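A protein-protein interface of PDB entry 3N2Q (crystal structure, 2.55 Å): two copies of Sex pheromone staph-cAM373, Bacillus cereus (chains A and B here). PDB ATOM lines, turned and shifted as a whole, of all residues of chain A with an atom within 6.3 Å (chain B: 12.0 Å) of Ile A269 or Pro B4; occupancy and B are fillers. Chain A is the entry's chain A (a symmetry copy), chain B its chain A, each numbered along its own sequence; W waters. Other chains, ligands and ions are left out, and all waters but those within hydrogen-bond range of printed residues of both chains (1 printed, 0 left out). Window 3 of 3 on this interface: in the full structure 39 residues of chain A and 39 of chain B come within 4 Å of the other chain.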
ATOM      1  N   SER A 143      27.763  32.562  20.973  1.00  0.00           N
ATOM      2  CA  SER A 143      26.684  31.579  21.146  1.00  0.00           C
ATOM      3  C   SER A 143      25.890  31.776  22.448  1.00  0.00           C
ATOM      4  O   SER A 143      25.034  30.960  22.798  1.00  0.00           O
ATOM      5  CB  SER A 143      27.236  30.151  21.053  1.00  0.00           C
ATOM      6  OG  SER A 143      28.249  29.949  22.010  1.00  0.00           O
ATOM      7  N   SER A 144      26.186  32.861  23.160  1.00  0.00           N
ATOM      8  CA  SER A 144      25.459  33.211  24.375  1.00  0.00           C
ATOM      9  C   SER A 144      24.300  34.166  24.071  1.00  0.00           C
ATOM     10  O   SER A 144      24.442  35.074  23.256  1.00  0.00           O
ATOM     11  CB  SER A 144      26.417  33.854  25.368  1.00  0.00           C
ATOM     12  OG  SER A 144      25.710  34.479  26.425  1.00  0.00           O
ATOM     13  N   LEU A 145      23.163  33.959  24.719  1.00  0.00           N
ATOM     14  CA  LEU A 145      22.046  34.892  24.601  1.00  0.00           C
ATOM     15  C   LEU A 145      22.245  36.227  25.369  1.00  0.00           C
ATOM     16  O   LEU A 145      21.633  37.229  25.008  1.00  0.00           O
ATOM     17  CB  LEU A 145      20.719  34.227  24.986  1.00  0.00           C
ATOM     18  CG  LEU A 145      20.225  33.032  24.175  1.00  0.00           C
ATOM     19  CD1 LEU A 145      19.000  32.407  24.810  1.00  0.00           C
ATOM     20  CD2 LEU A 145      19.923  33.405  22.747  1.00  0.00           C
ATOM     21  N   ASN A 227      12.671  34.271  35.795  1.00  0.00           N
ATOM     22  CA  ASN A 227      12.658  32.807  35.793  1.00  0.00           C
ATOM     23  C   ASN A 227      11.284  32.270  36.183  1.00  0.00           C
ATOM     24  O   ASN A 227      10.614  32.799  37.078  1.00  0.00           O
ATOM     25  CB  ASN A 227      13.704  32.255  36.765  1.00  0.00           C
ATOM     26  CG  ASN A 227      15.123  32.359  36.205  1.00  0.00           C
ATOM     27  OD1 ASN A 227      15.659  31.396  35.630  1.00  0.00           O
ATOM     28  ND2 ASN A 227      15.732  33.543  36.334  1.00  0.00           N
ATOM     29  N   GLN A 262      13.647  33.025  31.435  1.00  0.00           N
ATOM     30  CA  GLN A 262      14.033  31.630  31.298  1.00  0.00           C
ATOM     31  C   GLN A 262      12.892  30.784  31.789  1.00  0.00           C
ATOM     32  O   GLN A 262      12.365  31.024  32.875  1.00  0.00           O
ATOM     33  CB  GLN A 262      15.285  31.329  32.109  1.00  0.00           C
ATOM     34  CG  GLN A 262      16.462  32.208  31.758  1.00  0.00           C
ATOM     35  CD  GLN A 262      17.749  31.820  32.473  1.00  0.00           C
ATOM     36  OE1 GLN A 262      18.814  31.810  31.870  1.00  0.00           O
ATOM     37  NE2 GLN A 262      17.657  31.515  33.755  1.00  0.00           N
ATOM     38  N   ILE A 263      12.486  29.805  30.994  1.00  0.00           N
ATOM     39  CA  ILE A 263      11.454  28.868  31.435  1.00  0.00           C
ATOM     40  C   ILE A 263      12.129  27.553  31.784  1.00  0.00           C
ATOM     41  O   ILE A 263      12.683  26.874  30.909  1.00  0.00           O
ATOM     42  CB  ILE A 263      10.339  28.680  30.379  1.00  0.00           C
ATOM     43  CG1 ILE A 263       9.604  30.007  30.147  1.00  0.00           C
ATOM     44  CG2 ILE A 263       9.359  27.608  30.821  1.00  0.00           C
ATOM     45  CD1 ILE A 263       8.680  30.021  28.953  1.00  0.00           C
ATOM     46  N   LYS A 264      12.099  27.211  33.069  1.00  0.00           N
ATOM     47  CA  LYS A 264      12.790  26.029  33.582  1.00  0.00           C
ATOM     48  C   LYS A 264      11.810  24.911  33.932  1.00  0.00           C
ATOM     49  O   LYS A 264      10.637  25.159  34.188  1.00  0.00           O
ATOM     50  CB  LYS A 264      13.665  26.388  34.806  1.00  0.00           C
ATOM     51  CG  LYS A 264      14.483  27.686  34.665  1.00  0.00           C
ATOM     52  CD  LYS A 264      15.144  28.121  35.964  1.00  0.00           C
ATOM     53  CE  LYS A 264      16.513  27.460  36.117  1.00  0.00           C
ATOM     54  NZ  LYS A 264      17.241  27.918  37.333  1.00  0.00           N
ATOM     55  N   SER A 265      12.298  23.677  33.936  1.00  0.00           N
ATOM     56  CA  SER A 265      11.523  22.534  34.422  1.00  0.00           C
ATOM     57  C   SER A 265      12.405  21.322  34.507  1.00  0.00           C
ATOM     58  O   SER A 265      13.127  21.004  33.544  1.00  0.00           O
ATOM     59  CB  SER A 265      10.350  22.206  33.495  1.00  0.00           C
ATOM     60  OG  SER A 265      10.692  21.206  32.550  1.00  0.00           O
ATOM     61  N   SER A 267      15.072  20.575  36.462  1.00  0.00           N
ATOM     62  CA  SER A 267      16.491  20.954  36.469  1.00  0.00           C
ATOM     63  C   SER A 267      17.076  21.240  35.066  1.00  0.00           C
ATOM     64  O   SER A 267      18.191  20.807  34.752  1.00  0.00           O
ATOM     65  CB  SER A 267      17.329  19.902  37.224  1.00  0.00           C
ATOM     66  N   LYS A 268      16.314  21.970  34.245  1.00  0.00           N
ATOM     67  CA  LYS A 268      16.657  22.273  32.846  1.00  0.00           C
ATOM     68  C   LYS A 268      16.034  23.601  32.388  1.00  0.00           C
ATOM     69  O   LYS A 268      14.868  23.885  32.675  1.00  0.00           O
ATOM     70  CB  LYS A 268      16.129  21.182  31.919  1.00  0.00           C
ATOM     71  CG  LYS A 268      17.080  20.047  31.602  1.00  0.00           C
ATOM     72  CD  LYS A 268      16.366  18.943  30.807  1.00  0.00           C
ATOM     73  CE  LYS A 268      15.606  19.518  29.599  1.00  0.00           C
ATOM     74  NZ  LYS A 268      15.117  18.499  28.621  1.00  0.00           N
ATOM     75  N   ILE A 269      16.798  24.408  31.662  1.00  0.00           N
ATOM     76  CA  ILE A 269      16.209  25.575  31.008  1.00  0.00           C
ATOM     77  C   ILE A 269      15.675  25.181  29.626  1.00  0.00           C
ATOM     78  O   ILE A 269      16.436  24.843  28.730  1.00  0.00           O
ATOM     79  CB  ILE A 269      17.193  26.751  30.905  1.00  0.00           C
ATOM     80  CG1 ILE A 269      17.838  27.026  32.265  1.00  0.00           C
ATOM     81  CG2 ILE A 269      16.468  27.979  30.383  1.00  0.00           C
ATOM     82  CD1 ILE A 269      19.104  27.833  32.174  1.00  0.00           C
ATOM     83  N   GLU A 270      14.355  25.230  29.480  1.00  0.00           N
ATOM     84  CA  GLU A 270      13.663  24.647  28.346  1.00  0.00           C
ATOM     85  C   GLU A 270      13.485  25.649  27.179  1.00  0.00           C
ATOM     86  O   GLU A 270      13.574  25.272  25.992  1.00  0.00           O
ATOM     87  CB  GLU A 270      12.316  24.109  28.831  1.00  0.00           C
ATOM     88  CG  GLU A 270      11.910  22.795  28.198  1.00  0.00           C
ATOM     89  CD  GLU A 270      12.772  21.606  28.630  1.00  0.00           C
ATOM     90  OE1 GLU A 270      13.660  21.210  27.855  1.00  0.00           O
ATOM     91  OE2 GLU A 270      12.565  21.067  29.739  1.00  0.00           O
ATOM     92  N   ALA A 271      13.234  26.915  27.524  1.00  0.00           N
ATOM     93  CA  ALA A 271      13.166  28.002  26.546  1.00  0.00           C
ATOM     94  C   ALA A 271      13.587  29.323  27.182  1.00  0.00           C
ATOM     95  O   ALA A 271      13.473  29.488  28.402  1.00  0.00           O
ATOM     96  CB  ALA A 271      11.759  28.121  25.956  1.00  0.00           C
ATOM     97  N   VAL A 272      14.083  30.254  26.369  1.00  0.00           N
ATOM     98  CA  VAL A 272      14.429  31.597  26.843  1.00  0.00           C
ATOM     99  C   VAL A 272      13.854  32.642  25.905  1.00  0.00           C
ATOM    100  O   VAL A 272      14.108  32.595  24.701  1.00  0.00           O
ATOM    101  CB  VAL A 272      15.960  31.826  26.944  1.00  0.00           C
ATOM    102  CG1 VAL A 272      16.247  33.156  27.596  1.00  0.00           C
ATOM    103  CG2 VAL A 272      16.637  30.701  27.729  1.00  0.00           C
ATOM    104  N   SER A 285      14.268  31.041  21.981  1.00  0.00           N
ATOM    105  CA  SER A 285      15.205  29.935  21.727  1.00  0.00           C
ATOM    106  C   SER A 285      14.802  28.723  22.569  1.00  0.00           C
ATOM    107  O   SER A 285      14.528  28.841  23.765  1.00  0.00           O
ATOM    108  CB  SER A 285      16.648  30.310  22.080  1.00  0.00           C
ATOM    109  OG  SER A 285      17.151  31.343  21.263  1.00  0.00           O
ATOM    110  N   PHE A 286      14.783  27.555  21.940  1.00  0.00           N
ATOM    111  CA  PHE A 286      14.495  26.328  22.652  1.00  0.00           C
ATOM    112  C   PHE A 286      15.768  25.536  22.855  1.00  0.00           C
ATOM    113  O   PHE A 286      16.695  25.626  22.054  1.00  0.00           O
ATOM    114  CB  PHE A 286      13.426  25.513  21.919  1.00  0.00           C
ATOM    115  CG  PHE A 286      12.080  26.185  21.888  1.00  0.00           C
ATOM    116  CD1 PHE A 286      11.187  26.040  22.949  1.00  0.00           C
ATOM    117  CD2 PHE A 286      11.709  26.981  20.813  1.00  0.00           C
ATOM    118  CE1 PHE A 286       9.929  26.674  22.935  1.00  0.00           C
ATOM    119  CE2 PHE A 286      10.451  27.619  20.790  1.00  0.00           C
ATOM    120  CZ  PHE A 286       9.564  27.465  21.860  1.00  0.00           C
ATOM    121  N   LEU A 287      15.808  24.780  23.947  1.00  0.00           N
ATOM    122  CA  LEU A 287      16.898  23.854  24.222  1.00  0.00           C
ATOM    123  C   LEU A 287      17.142  22.904  23.053  1.00  0.00           C
ATOM    124  O   LEU A 287      18.291  22.714  22.640  1.00  0.00           O
ATOM    125  CB  LEU A 287      16.605  23.051  25.494  1.00  0.00           C
ATOM    126  CG  LEU A 287      17.746  22.203  26.065  1.00  0.00           C
ATOM    127  CD1 LEU A 287      19.043  23.015  26.225  1.00  0.00           C
ATOM    128  CD2 LEU A 287      17.326  21.605  27.391  1.00  0.00           C
ATOM    129  OXT LEU A 287      16.202  22.318  22.504  1.00  0.00           O
ATOM    130  N   ASN B   2      23.159  24.405  31.704  1.00  0.00           N
ATOM    131  CA  ASN B   2      23.313  24.643  30.242  1.00  0.00           C
ATOM    132  C   ASN B   2      22.025  25.226  29.625  1.00  0.00           C
ATOM    133  O   ASN B   2      20.999  24.543  29.532  1.00  0.00           O
ATOM    134  CB  ASN B   2      23.730  23.347  29.534  1.00  0.00           C
ATOM    135  N   ALA B   3      22.093  26.490  29.212  1.00  0.00           N
ATOM    136  CA  ALA B   3      20.952  27.208  28.626  1.00  0.00           C
ATOM    137  C   ALA B   3      20.961  27.158  27.097  1.00  0.00           C
ATOM    138  O   ALA B   3      22.035  27.187  26.488  1.00  0.00           O
ATOM    139  CB  ALA B   3      20.959  28.667  29.094  1.00  0.00           C
ATOM    140  N   PRO B   4      19.768  27.115  26.459  1.00  0.00           N
ATOM    141  CA  PRO B   4      19.772  27.111  24.995  1.00  0.00           C
ATOM    142  C   PRO B   4      20.679  28.199  24.448  1.00  0.00           C
ATOM    143  O   PRO B   4      20.891  29.227  25.095  1.00  0.00           O
ATOM    144  CB  PRO B   4      18.307  27.389  24.615  1.00  0.00           C
ATOM    145  CG  PRO B   4      17.610  27.733  25.876  1.00  0.00           C
ATOM    146  CD  PRO B   4      18.396  27.117  26.993  1.00  0.00           C
ATOM    147  N   LEU B   5      21.221  27.960  23.262  1.00  0.00           N
ATOM    148  CA  LEU B   5      22.195  28.867  22.681  1.00  0.00           C
ATOM    149  C   LEU B   5      21.552  29.806  21.674  1.00  0.00           C
ATOM    150  O   LEU B   5      20.441  29.567  21.194  1.00  0.00           O
ATOM    151  CB  LEU B   5      23.353  28.078  22.052  1.00  0.00           C
ATOM    152  CG  LEU B   5      24.094  27.084  22.966  1.00  0.00           C
ATOM    153  CD1 LEU B   5      24.992  26.159  22.141  1.00  0.00           C
ATOM    154  CD2 LEU B   5      24.887  27.783  24.069  1.00  0.00           C
ATOM    155  N   LYS B   6      22.254  30.896  21.398  1.00  0.00           N
ATOM    156  CA  LYS B   6      21.914  31.767  20.298  1.00  0.00           C
ATOM    157  C   LYS B   6      22.125  30.959  19.040  1.00  0.00           C
ATOM    158  O   LYS B   6      23.214  30.439  18.806  1.00  0.00           O
ATOM    159  CB  LYS B   6      22.820  32.997  20.287  1.00  0.00           C
ATOM    160  CG  LYS B   6      22.124  34.245  19.823  1.00  0.00           C
ATOM    161  CD  LYS B   6      23.099  35.364  19.537  1.00  0.00           C
ATOM    162  CE  LYS B   6      22.357  36.565  18.938  1.00  0.00           C
ATOM    163  NZ  LYS B   6      23.294  37.586  18.341  1.00  0.00           N
ATOM    164  N   GLU B   7      21.059  30.824  18.257  1.00  0.00           N
ATOM    165  CA  GLU B   7      21.105  30.073  17.009  1.00  0.00           C
ATOM    166  C   GLU B   7      21.394  30.962  15.793  1.00  0.00           C
ATOM    167  O   GLU B   7      21.707  30.457  14.712  1.00  0.00           O
ATOM    168  CB  GLU B   7      19.849  29.209  16.816  1.00  0.00           C
ATOM    169  CG  GLU B   7      18.672  29.489  17.762  1.00  0.00           C
ATOM    170  CD  GLU B   7      17.627  28.366  17.793  1.00  0.00           C
ATOM    171  OE1 GLU B   7      17.824  27.328  17.131  1.00  0.00           O
ATOM    172  OE2 GLU B   7      16.598  28.519  18.486  1.00  0.00           O
ATOM    173  N   GLN B   8      21.325  32.279  15.984  1.00  0.00           N
ATOM    174  CA  GLN B   8      21.690  33.223  14.944  1.00  0.00           C
ATOM    175  C   GLN B   8      23.025  33.890  15.257  1.00  0.00           C
ATOM    176  O   GLN B   8      23.105  34.763  16.131  1.00  0.00           O
ATOM    177  CB  GLN B   8      20.606  34.287  14.773  1.00  0.00           C
ATOM    178  CG  GLN B   8      20.976  35.394  13.793  1.00  0.00           C
ATOM    179  CD  GLN B   8      19.925  36.488  13.725  1.00  0.00           C
ATOM    180  OE1 GLN B   8      18.872  36.316  13.090  1.00  0.00           O
ATOM    181  NE2 GLN B   8      20.205  37.628  14.380  1.00  0.00           N
ATOM    182  N   LYS B   9      24.066  33.480  14.539  1.00  0.00           N
ATOM    183  CA  LYS B   9      25.385  34.093  14.677  1.00  0.00           C
ATOM    184  C   LYS B   9      25.745  34.932  13.441  1.00  0.00           C
ATOM    185  O   LYS B   9      25.273  34.672  12.336  1.00  0.00           O
ATOM    186  CB  LYS B   9      26.435  33.021  14.986  1.00  0.00           C
ATOM    187  CG  LYS B   9      26.131  32.254  16.310  1.00  0.00           C
ATOM    188  CD  LYS B   9      27.343  31.544  16.896  1.00  0.00           C
ATOM    189  CE  LYS B   9      27.538  30.142  16.321  1.00  0.00           C
ATOM    190  NZ  LYS B   9      28.220  29.257  17.323  1.00  0.00           N
ATOM    191  N   LEU B  46       8.368  34.675  17.499  1.00  0.00           N
ATOM    192  CA  LEU B  46       9.560  34.823  16.666  1.00  0.00           C
ATOM    193  C   LEU B  46      10.674  33.877  17.106  1.00  0.00           C
ATOM    194  O   LEU B  46      11.095  33.888  18.276  1.00  0.00           O
ATOM    195  CB  LEU B  46      10.052  36.282  16.646  1.00  0.00           C
ATOM    196  CG  LEU B  46      11.418  36.560  15.980  1.00  0.00           C
ATOM    197  CD1 LEU B  46      11.433  36.152  14.527  1.00  0.00           C
ATOM    198  CD2 LEU B  46      11.883  38.013  16.123  1.00  0.00           C
ATOM    199  N   GLN B  47      11.126  33.054  16.163  1.00  0.00           N
ATOM    200  CA  GLN B  47      12.339  32.250  16.314  1.00  0.00           C
ATOM    201  C   GLN B  47      13.350  32.553  15.198  1.00  0.00           C
ATOM    202  O   GLN B  47      12.987  32.985  14.090  1.00  0.00           O
ATOM    203  CB  GLN B  47      12.035  30.754  16.310  1.00  0.00           C
ATOM    204  CG  GLN B  47      11.172  30.253  17.439  1.00  0.00           C
ATOM    205  CD  GLN B  47      11.121  28.724  17.489  1.00  0.00           C
ATOM    206  OE1 GLN B  47      12.097  28.080  17.872  1.00  0.00           O
ATOM    207  NE2 GLN B  47       9.984  28.143  17.115  1.00  0.00           N
ATOM    208  N   LEU B  48      14.618  32.277  15.481  1.00  0.00           N
ATOM    209  CA  LEU B  48      15.697  32.622  14.580  1.00  0.00           C
ATOM    210  C   LEU B  48      16.320  31.409  13.895  1.00  0.00           C
ATOM    211  O   LEU B  48      16.568  30.370  14.531  1.00  0.00           O
ATOM    212  CB  LEU B  48      16.772  33.401  15.333  1.00  0.00           C
ATOM    213  CG  LEU B  48      16.354  34.657  16.109  1.00  0.00           C
ATOM    214  CD1 LEU B  48      17.604  35.339  16.675  1.00  0.00           C
ATOM    215  CD2 LEU B  48      15.567  35.620  15.244  1.00  0.00           C
ATOM    216  N   GLN B  50      15.762  28.910  11.641  1.00  0.00           N
ATOM    217  CA  GLN B  50      15.248  27.549  11.799  1.00  0.00           C
ATOM    218  C   GLN B  50      15.497  26.621  10.604  1.00  0.00           C
ATOM    219  O   GLN B  50      15.632  25.418  10.778  1.00  0.00           O
ATOM    220  CB  GLN B  50      13.757  27.565  12.146  1.00  0.00           C
ATOM    221  CG  GLN B  50      13.443  28.179  13.502  1.00  0.00           C
ATOM    222  CD  GLN B  50      14.021  27.392  14.667  1.00  0.00           C
ATOM    223  OE1 GLN B  50      14.960  27.842  15.323  1.00  0.00           O
ATOM    224  NE2 GLN B  50      13.464  26.217  14.930  1.00  0.00           N
HETATM  225  O   HOH W   1      18.070  31.973  19.132  1.00  0.00           O
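Water W1 lies within hydrogen-bond range of OG of Ser A285 (2.4 Å) and N of Glu B7 (3.3 Å).
No position is printed for both chains.
Of the 15 pairs that touch across the chains among the printed residues, none has its exchanged pair printed and touching as well.
Leu B5 touches Ser A143.
CB of Ser A143 touches NZ of Lys B9, 3.96 Å away.
Leu A145 touches Pro B4 (CD1 to O, 3.7 Å).
Leu A145 touches Lys B6 (CD2 to CA, 3.6 Å).
CB of Ala B3 touches CD1 of Ile A269, 3.7 Å away.
Ile A269 touches Pro B4.
Val A272 touches Pro B4 (CG2 to CG, 3.6 Å).
Pro B4 touches Ser A285.
Ser A285 touches Glu B7 (CA to OE2, 3.8 Å).
Gln B47 touches Phe A286.
Hydrophobic or aromatic side chains of chain B within 4 Å of the printed part of chain A: Ala B3, Pro B4 and Leu B5.
Of the 17 printed residues of chain A, 8 touch a printed residue of chain B.
Among the printed residues, no Asp or Glu carboxylate lies within 4 Å of a Lys or Arg side-chain nitrogen of the other chain.
OE1 of Glu B7 lies close to OE1 of Gln B50.
O of Glu A270 is in hydrogen-bond range of N of Leu A287 (3.1 Å).
O of Ser A285 lies within hydrogen-bond range of N of Val A272 (3.0 Å).
N of Lys B6 lies within hydrogen-bond range of O of Ser A143 (3.1 Å).
Of chain A, only Leu A145, Ile A269, Val A272, Ser A285, Phe A286 and Leu A287 come within 4 Å of Pro B4.
Printed residues of chain B within 4 Å of Ser A144: Lys B6.
No residue of chain B comes within 4 Å of Gln A262.
Lys A264 touches none of the printed residues of chain B.
No residue of chain B comes within 4 Å of Ser A265.
No residue of chain B comes within 4 Å of Glu A270.
Val A272 touches just one residue of chain B: Pro B4 (3.6 Å).
Ser A285 touches just these residues of chain B: Pro B4, Leu B5 and Glu B7.
Printed residues of chain A within 4 Å of Ala B3: Ile A269 (3.7 Å).
Printed residues of chain A within 4 Å of Gln B47: Phe A286 (3.2 Å).
Printed residues of chain B within 4 Å of Phe A286: Pro B4 and Gln B47.
Of the printed residues of chain B, Leu A145 touches Pro B4 and Lys B6.
Printed residues of chain A within 4 Å of Lys B9: Ser A143.
The nearest residue of chain A that does not touch Pro B4 is Ala A271 (4.5 Å).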
